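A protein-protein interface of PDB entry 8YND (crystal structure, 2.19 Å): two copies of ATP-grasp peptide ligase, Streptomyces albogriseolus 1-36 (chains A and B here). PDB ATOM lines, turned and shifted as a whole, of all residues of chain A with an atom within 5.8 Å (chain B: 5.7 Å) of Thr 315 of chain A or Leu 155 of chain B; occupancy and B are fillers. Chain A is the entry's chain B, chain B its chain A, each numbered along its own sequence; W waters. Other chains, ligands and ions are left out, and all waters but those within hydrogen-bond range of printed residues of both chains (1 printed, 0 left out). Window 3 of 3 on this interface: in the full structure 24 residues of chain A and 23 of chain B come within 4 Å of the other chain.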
ATOM      1  N   ILE A 310     -21.332 -10.291  39.694  1.00  0.00           N
ATOM      2  CA  ILE A 310     -20.371 -10.578  38.638  1.00  0.00           C
ATOM      3  C   ILE A 310     -21.100 -10.925  37.349  1.00  0.00           C
ATOM      4  O   ILE A 310     -20.676 -10.540  36.249  1.00  0.00           O
ATOM      5  CB  ILE A 310     -19.421 -11.702  39.091  1.00  0.00           C
ATOM      6  CG1 ILE A 310     -18.531 -11.219  40.246  1.00  0.00           C
ATOM      7  CG2 ILE A 310     -18.563 -12.192  37.938  1.00  0.00           C
ATOM      8  CD1 ILE A 310     -17.465 -10.203  39.851  1.00  0.00           C
ATOM      9  N   GLU A 311     -22.215 -11.642  37.466  1.00  0.00           N
ATOM     10  CA  GLU A 311     -23.038 -11.951  36.307  1.00  0.00           C
ATOM     11  C   GLU A 311     -23.547 -10.684  35.655  1.00  0.00           C
ATOM     12  O   GLU A 311     -23.668 -10.611  34.427  1.00  0.00           O
ATOM     13  CB  GLU A 311     -24.212 -12.845  36.723  1.00  0.00           C
ATOM     14  CG  GLU A 311     -24.811 -13.662  35.601  1.00  0.00           C
ATOM     15  CD  GLU A 311     -23.762 -14.444  34.814  1.00  0.00           C
ATOM     16  OE1 GLU A 311     -22.879 -15.072  35.458  1.00  0.00           O
ATOM     17  OE2 GLU A 311     -23.841 -14.438  33.560  1.00  0.00           O
ATOM     18  N   MET A 312     -23.843  -9.670  36.455  1.00  0.00           N
ATOM     19  CA  MET A 312     -24.256  -8.408  35.872  1.00  0.00           C
ATOM     20  C   MET A 312     -23.077  -7.692  35.218  1.00  0.00           C
ATOM     21  O   MET A 312     -23.259  -7.000  34.209  1.00  0.00           O
ATOM     22  CB  MET A 312     -24.908  -7.553  36.950  1.00  0.00           C
ATOM     23  CG  MET A 312     -25.685  -6.373  36.425  1.00  0.00           C
ATOM     24  SD  MET A 312     -25.354  -5.018  37.540  1.00  0.00           S
ATOM     25  CE  MET A 312     -23.580  -4.924  37.274  1.00  0.00           C
ATOM     26  N   ILE A 313     -21.865  -7.859  35.766  1.00  0.00           N
ATOM     27  CA  ILE A 313     -20.666  -7.351  35.102  1.00  0.00           C
ATOM     28  C   ILE A 313     -20.529  -7.992  33.730  1.00  0.00           C
ATOM     29  O   ILE A 313     -20.284  -7.318  32.728  1.00  0.00           O
ATOM     30  CB  ILE A 313     -19.409  -7.610  35.963  1.00  0.00           C
ATOM     31  CG1 ILE A 313     -19.375  -6.728  37.207  1.00  0.00           C
ATOM     32  CG2 ILE A 313     -18.183  -7.352  35.172  1.00  0.00           C
ATOM     33  CD1 ILE A 313     -19.386  -5.268  36.890  1.00  0.00           C
ATOM     34  N   ARG A 314     -20.687  -9.310  33.673  1.00  0.00           N
ATOM     35  CA  ARG A 314     -20.633 -10.028  32.406  1.00  0.00           C
ATOM     36  C   ARG A 314     -21.709  -9.532  31.437  1.00  0.00           C
ATOM     37  O   ARG A 314     -21.434  -9.307  30.249  1.00  0.00           O
ATOM     38  CB  ARG A 314     -20.797 -11.529  32.659  1.00  0.00           C
ATOM     39  CG  ARG A 314     -20.294 -12.429  31.532  1.00  0.00           C
ATOM     40  CD  ARG A 314     -20.376 -13.912  31.933  1.00  0.00           C
ATOM     41  NE  ARG A 314     -21.760 -14.359  31.935  1.00  0.00           N
ATOM     42  CZ  ARG A 314     -22.454 -14.659  30.844  1.00  0.00           C
ATOM     43  NH1 ARG A 314     -21.900 -14.647  29.644  1.00  0.00           N
ATOM     44  NH2 ARG A 314     -23.735 -14.973  30.958  1.00  0.00           N
ATOM     45  N   THR A 315     -22.942  -9.373  31.925  1.00  0.00           N
ATOM     46  CA  THR A 315     -24.025  -8.865  31.078  1.00  0.00           C
ATOM     47  C   THR A 315     -23.656  -7.512  30.463  1.00  0.00           C
ATOM     48  O   THR A 315     -23.956  -7.245  29.291  1.00  0.00           O
ATOM     49  CB  THR A 315     -25.313  -8.758  31.906  1.00  0.00           C
ATOM     50  OG1 THR A 315     -25.712 -10.066  32.334  1.00  0.00           O
ATOM     51  CG2 THR A 315     -26.467  -8.109  31.098  1.00  0.00           C
ATOM     52  N   ILE A 316     -22.987  -6.653  31.237  1.00  0.00           N
ATOM     53  CA  ILE A 316     -22.578  -5.342  30.747  1.00  0.00           C
ATOM     54  C   ILE A 316     -21.590  -5.474  29.590  1.00  0.00           C
ATOM     55  O   ILE A 316     -21.547  -4.620  28.700  1.00  0.00           O
ATOM     56  CB  ILE A 316     -21.987  -4.523  31.913  1.00  0.00           C
ATOM     57  CG1 ILE A 316     -23.094  -4.008  32.850  1.00  0.00           C
ATOM     58  CG2 ILE A 316     -21.177  -3.340  31.404  1.00  0.00           C
ATOM     59  CD1 ILE A 316     -22.554  -3.347  34.128  1.00  0.00           C
ATOM     60  N   GLY A 317     -20.789  -6.542  29.574  1.00  0.00           N
ATOM     61  CA  GLY A 317     -19.882  -6.751  28.465  1.00  0.00           C
ATOM     62  C   GLY A 317     -18.437  -7.052  28.833  1.00  0.00           C
ATOM     63  O   GLY A 317     -17.644  -7.363  27.950  1.00  0.00           O
ATOM     64  N   TYR A 318     -18.056  -6.984  30.103  1.00  0.00           N
ATOM     65  CA  TYR A 318     -16.676  -7.282  30.429  1.00  0.00           C
ATOM     66  C   TYR A 318     -16.367  -8.747  30.164  1.00  0.00           C
ATOM     67  O   TYR A 318     -17.117  -9.648  30.564  1.00  0.00           O
ATOM     68  CB  TYR A 318     -16.366  -6.955  31.876  1.00  0.00           C
ATOM     69  CG  TYR A 318     -14.922  -7.203  32.184  1.00  0.00           C
ATOM     70  CD1 TYR A 318     -13.935  -6.369  31.685  1.00  0.00           C
ATOM     71  CD2 TYR A 318     -14.534  -8.292  32.941  1.00  0.00           C
ATOM     72  CE1 TYR A 318     -12.588  -6.600  31.966  1.00  0.00           C
ATOM     73  CE2 TYR A 318     -13.191  -8.528  33.229  1.00  0.00           C
ATOM     74  CZ  TYR A 318     -12.230  -7.677  32.740  1.00  0.00           C
ATOM     75  OH  TYR A 318     -10.902  -7.918  33.009  1.00  0.00           O
ATOM     76  N   ARG A 319     -15.267  -8.972  29.467  1.00  0.00           N
ATOM     77  CA  ARG A 319     -14.716 -10.293  29.216  1.00  0.00           C
ATOM     78  C   ARG A 319     -13.288 -10.310  29.740  1.00  0.00           C
ATOM     79  O   ARG A 319     -12.514  -9.392  29.462  1.00  0.00           O
ATOM     80  CB  ARG A 319     -14.731 -10.624  27.725  1.00  0.00           C
ATOM     81  CG  ARG A 319     -16.067 -10.430  27.062  1.00  0.00           C
ATOM     82  CD  ARG A 319     -17.015 -11.514  27.482  1.00  0.00           C
ATOM     83  NE  ARG A 319     -18.374 -11.341  26.966  1.00  0.00           N
ATOM     84  CZ  ARG A 319     -19.381 -10.845  27.674  1.00  0.00           C
ATOM     85  NH1 ARG A 319     -19.194 -10.340  28.880  1.00  0.00           N
ATOM     86  NH2 ARG A 319     -20.608 -10.871  27.168  1.00  0.00           N
ATOM     87  N   ARG B 150     -20.124   2.955  26.289  1.00  0.00           N
ATOM     88  CA  ARG B 150     -19.492   1.781  26.890  1.00  0.00           C
ATOM     89  C   ARG B 150     -20.495   0.654  27.101  1.00  0.00           C
ATOM     90  O   ARG B 150     -20.292  -0.481  26.639  1.00  0.00           O
ATOM     91  CB  ARG B 150     -18.855   2.181  28.218  1.00  0.00           C
ATOM     92  CG  ARG B 150     -17.540   2.935  28.079  1.00  0.00           C
ATOM     93  CD  ARG B 150     -17.278   3.694  29.370  1.00  0.00           C
ATOM     94  NE  ARG B 150     -16.023   4.432  29.340  1.00  0.00           N
ATOM     95  CZ  ARG B 150     -15.609   5.279  30.278  1.00  0.00           C
ATOM     96  NH1 ARG B 150     -16.370   5.606  31.311  1.00  0.00           N
ATOM     97  NH2 ARG B 150     -14.398   5.809  30.177  1.00  0.00           N
ATOM     98  N   LEU B 151     -21.592   0.947  27.805  1.00  0.00           N
ATOM     99  CA  LEU B 151     -22.613  -0.073  28.035  1.00  0.00           C
ATOM    100  C   LEU B 151     -23.100  -0.666  26.718  1.00  0.00           C
ATOM    101  O   LEU B 151     -23.191  -1.892  26.564  1.00  0.00           O
ATOM    102  CB  LEU B 151     -23.785   0.519  28.823  1.00  0.00           C
ATOM    103  CG  LEU B 151     -23.393   1.094  30.185  1.00  0.00           C
ATOM    104  CD1 LEU B 151     -24.608   1.655  30.915  1.00  0.00           C
ATOM    105  CD2 LEU B 151     -22.679   0.046  31.046  1.00  0.00           C
ATOM    106  N   ALA B 152     -23.385   0.195  25.743  1.00  0.00           N
ATOM    107  CA  ALA B 152     -23.923  -0.282  24.473  1.00  0.00           C
ATOM    108  C   ALA B 152     -22.898  -1.100  23.701  1.00  0.00           C
ATOM    109  O   ALA B 152     -23.251  -2.097  23.054  1.00  0.00           O
ATOM    110  CB  ALA B 152     -24.401   0.900  23.634  1.00  0.00           C
ATOM    111  N   ALA B 153     -21.627  -0.689  23.744  1.00  0.00           N
ATOM    112  CA  ALA B 153     -20.598  -1.487  23.093  1.00  0.00           C
ATOM    113  C   ALA B 153     -20.429  -2.823  23.803  1.00  0.00           C
ATOM    114  O   ALA B 153     -20.234  -3.859  23.158  1.00  0.00           O
ATOM    115  CB  ALA B 153     -19.283  -0.713  23.051  1.00  0.00           C
ATOM    116  N   GLY B 154     -20.530  -2.829  25.128  1.00  0.00           N
ATOM    117  CA  GLY B 154     -20.493  -4.097  25.837  1.00  0.00           C
ATOM    118  C   GLY B 154     -21.694  -4.971  25.535  1.00  0.00           C
ATOM    119  O   GLY B 154     -21.571  -6.184  25.367  1.00  0.00           O
ATOM    120  N   LEU B 155     -22.870  -4.368  25.435  1.00  0.00           N
ATOM    121  CA  LEU B 155     -24.061  -5.190  25.262  1.00  0.00           C
ATOM    122  C   LEU B 155     -24.220  -5.674  23.829  1.00  0.00           C
ATOM    123  O   LEU B 155     -24.841  -6.715  23.603  1.00  0.00           O
ATOM    124  CB  LEU B 155     -25.304  -4.406  25.687  1.00  0.00           C
ATOM    125  CG  LEU B 155     -26.573  -5.237  25.798  1.00  0.00           C
ATOM    126  CD1 LEU B 155     -26.366  -6.363  26.799  1.00  0.00           C
ATOM    127  CD2 LEU B 155     -27.778  -4.354  26.160  1.00  0.00           C
ATOM    128  N   GLY B 156     -23.662  -4.952  22.863  1.00  0.00           N
ATOM    129  CA  GLY B 156     -23.917  -5.210  21.467  1.00  0.00           C
ATOM    130  C   GLY B 156     -25.034  -4.386  20.871  1.00  0.00           C
ATOM    131  O   GLY B 156     -25.632  -4.812  19.876  1.00  0.00           O
ATOM    132  N   THR B 157     -25.348  -3.242  21.451  1.00  0.00           N
ATOM    133  CA  THR B 157     -26.402  -2.401  20.919  1.00  0.00           C
ATOM    134  C   THR B 157     -25.868  -1.619  19.722  1.00  0.00           C
ATOM    135  O   THR B 157     -24.775  -1.057  19.803  1.00  0.00           O
ATOM    136  CB  THR B 157     -26.907  -1.449  22.011  1.00  0.00           C
ATOM    137  OG1 THR B 157     -27.214  -2.197  23.197  1.00  0.00           O
ATOM    138  CG2 THR B 157     -28.127  -0.706  21.568  1.00  0.00           C
ATOM    139  N   PRO B 305     -33.612  -4.365  19.967  1.00  0.00           N
ATOM    140  CA  PRO B 305     -32.362  -3.917  20.620  1.00  0.00           C
ATOM    141  C   PRO B 305     -32.588  -2.836  21.667  1.00  0.00           C
ATOM    142  O   PRO B 305     -31.887  -2.812  22.686  1.00  0.00           O
ATOM    143  CB  PRO B 305     -31.506  -3.385  19.458  1.00  0.00           C
ATOM    144  CG  PRO B 305     -32.435  -3.174  18.352  1.00  0.00           C
ATOM    145  CD  PRO B 305     -33.568  -4.142  18.516  1.00  0.00           C
ATOM    146  N   GLU B 308     -33.672  -4.652  24.794  1.00  0.00           N
ATOM    147  CA  GLU B 308     -32.574  -5.335  25.459  1.00  0.00           C
ATOM    148  C   GLU B 308     -31.735  -4.348  26.256  1.00  0.00           C
ATOM    149  O   GLU B 308     -31.321  -4.638  27.385  1.00  0.00           O
ATOM    150  CB  GLU B 308     -31.700  -6.085  24.445  1.00  0.00           C
ATOM    151  CG  GLU B 308     -30.441  -6.593  25.107  1.00  0.00           C
ATOM    152  CD  GLU B 308     -29.692  -7.664  24.325  1.00  0.00           C
ATOM    153  OE1 GLU B 308     -28.954  -7.276  23.401  1.00  0.00           O
ATOM    154  OE2 GLU B 308     -29.783  -8.869  24.662  1.00  0.00           O
ATOM    155  N   PHE B 309     -31.494  -3.164  25.696  1.00  0.00           N
ATOM    156  CA  PHE B 309     -30.638  -2.213  26.386  1.00  0.00           C
ATOM    157  C   PHE B 309     -31.334  -1.655  27.626  1.00  0.00           C
ATOM    158  O   PHE B 309     -30.722  -1.567  28.697  1.00  0.00           O
ATOM    159  CB  PHE B 309     -30.204  -1.096  25.442  1.00  0.00           C
ATOM    160  CG  PHE B 309     -29.211  -0.176  26.061  1.00  0.00           C
ATOM    161  CD1 PHE B 309     -29.630   0.910  26.820  1.00  0.00           C
ATOM    162  CD2 PHE B 309     -27.862  -0.443  25.964  1.00  0.00           C
ATOM    163  CE1 PHE B 309     -28.707   1.733  27.441  1.00  0.00           C
ATOM    164  CE2 PHE B 309     -26.929   0.389  26.574  1.00  0.00           C
ATOM    165  CZ  PHE B 309     -27.350   1.475  27.309  1.00  0.00           C
ATOM    166  N   MET B 312     -31.385  -3.902  30.527  1.00  0.00           N
ATOM    167  CA  MET B 312     -30.121  -3.926  31.249  1.00  0.00           C
ATOM    168  C   MET B 312     -29.949  -2.712  32.149  1.00  0.00           C
ATOM    169  O   MET B 312     -29.372  -2.838  33.240  1.00  0.00           O
ATOM    170  CB  MET B 312     -28.936  -4.008  30.288  1.00  0.00           C
ATOM    171  CG  MET B 312     -27.692  -3.341  30.840  1.00  0.00           C
ATOM    172  SD  MET B 312     -26.231  -3.708  29.894  1.00  0.00           S
ATOM    173  CE  MET B 312     -26.165  -2.153  29.001  1.00  0.00           C
HETATM  174  O   HOH W   1     -18.827  -8.223  25.256  1.00  0.00           O
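Of the 12 printed residues of chain B, 3 touch a printed residue of chain A. Printed residues of chain B that touch a printed residue of chain A: Leu 151, Gly 154 and Leu 155. Hydrophobic or aromatic side chains of chain B within 4 Å of the printed part of chain A: Leu 151 and Leu 155. Of the 10 printed residues of chain A, 3 touch a printed residue of chain B. Among the printed residues, 5 pairs touch across the chains. Among the printed residues, no Asp or Glu carboxylate lies within 4 Å of a Lys or Arg side-chain nitrogen of the other chain.
Water W1 bridges the backbone carbonyl oxygen (O) of Gly 317 of chain A (3.1 Å) and the backbone carbonyl oxygen (O) of Gly 154 of chain B (3.4 Å).
1 position is printed for both chains. Of the 5 pairs that touch across the chains among the printed residues, none has its exchanged pair printed and touching as well.
Thr 315 of chain A touches one residue of chain B. Leu 155 of chain B touches just these residues of chain A: Thr 315 and Ile 316. Of the printed residues of chain A, Leu 151 of chain B touches Ile 316. Of the printed residues of chain B, Gly 317 of chain A touches Gly 154. Arg 314 of chain A touches none of the printed residues of chain B. Ile 313 of chain A touches none of the printed residues of chain B. The nearest residue of chain A that does not touch Leu 155 of chain B is Gly 317 of chain A (4.9 Å).
Thr 315 of chain A touches Leu 155 of chain B (O to CD1, 3.6 Å). CD2 of Leu 151 of chain B touches CG2 of Ile 316 of chain A, 3.7 Å away. CA of Gly 154 of chain B touches O of Ile 316 of chain A, at 3.1 Å. N of Leu 155 of chain B touches O of Ile 316 of chain A, at 3.5 Å. Gly 317 of chain A touches Gly 154 of chain B.
The side-chain hydroxyl (OG1) of Thr 315 of chain A lies within hydrogen-bond range of the backbone carbonyl oxygen (O) of Glu 311 of chain A (3.0 Å). The guanidinium group (NH1) of Arg 319 of chain A sits close to the backbone carbonyl oxygen (O) of Gly 317 of chain A, 3.5 Å away.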
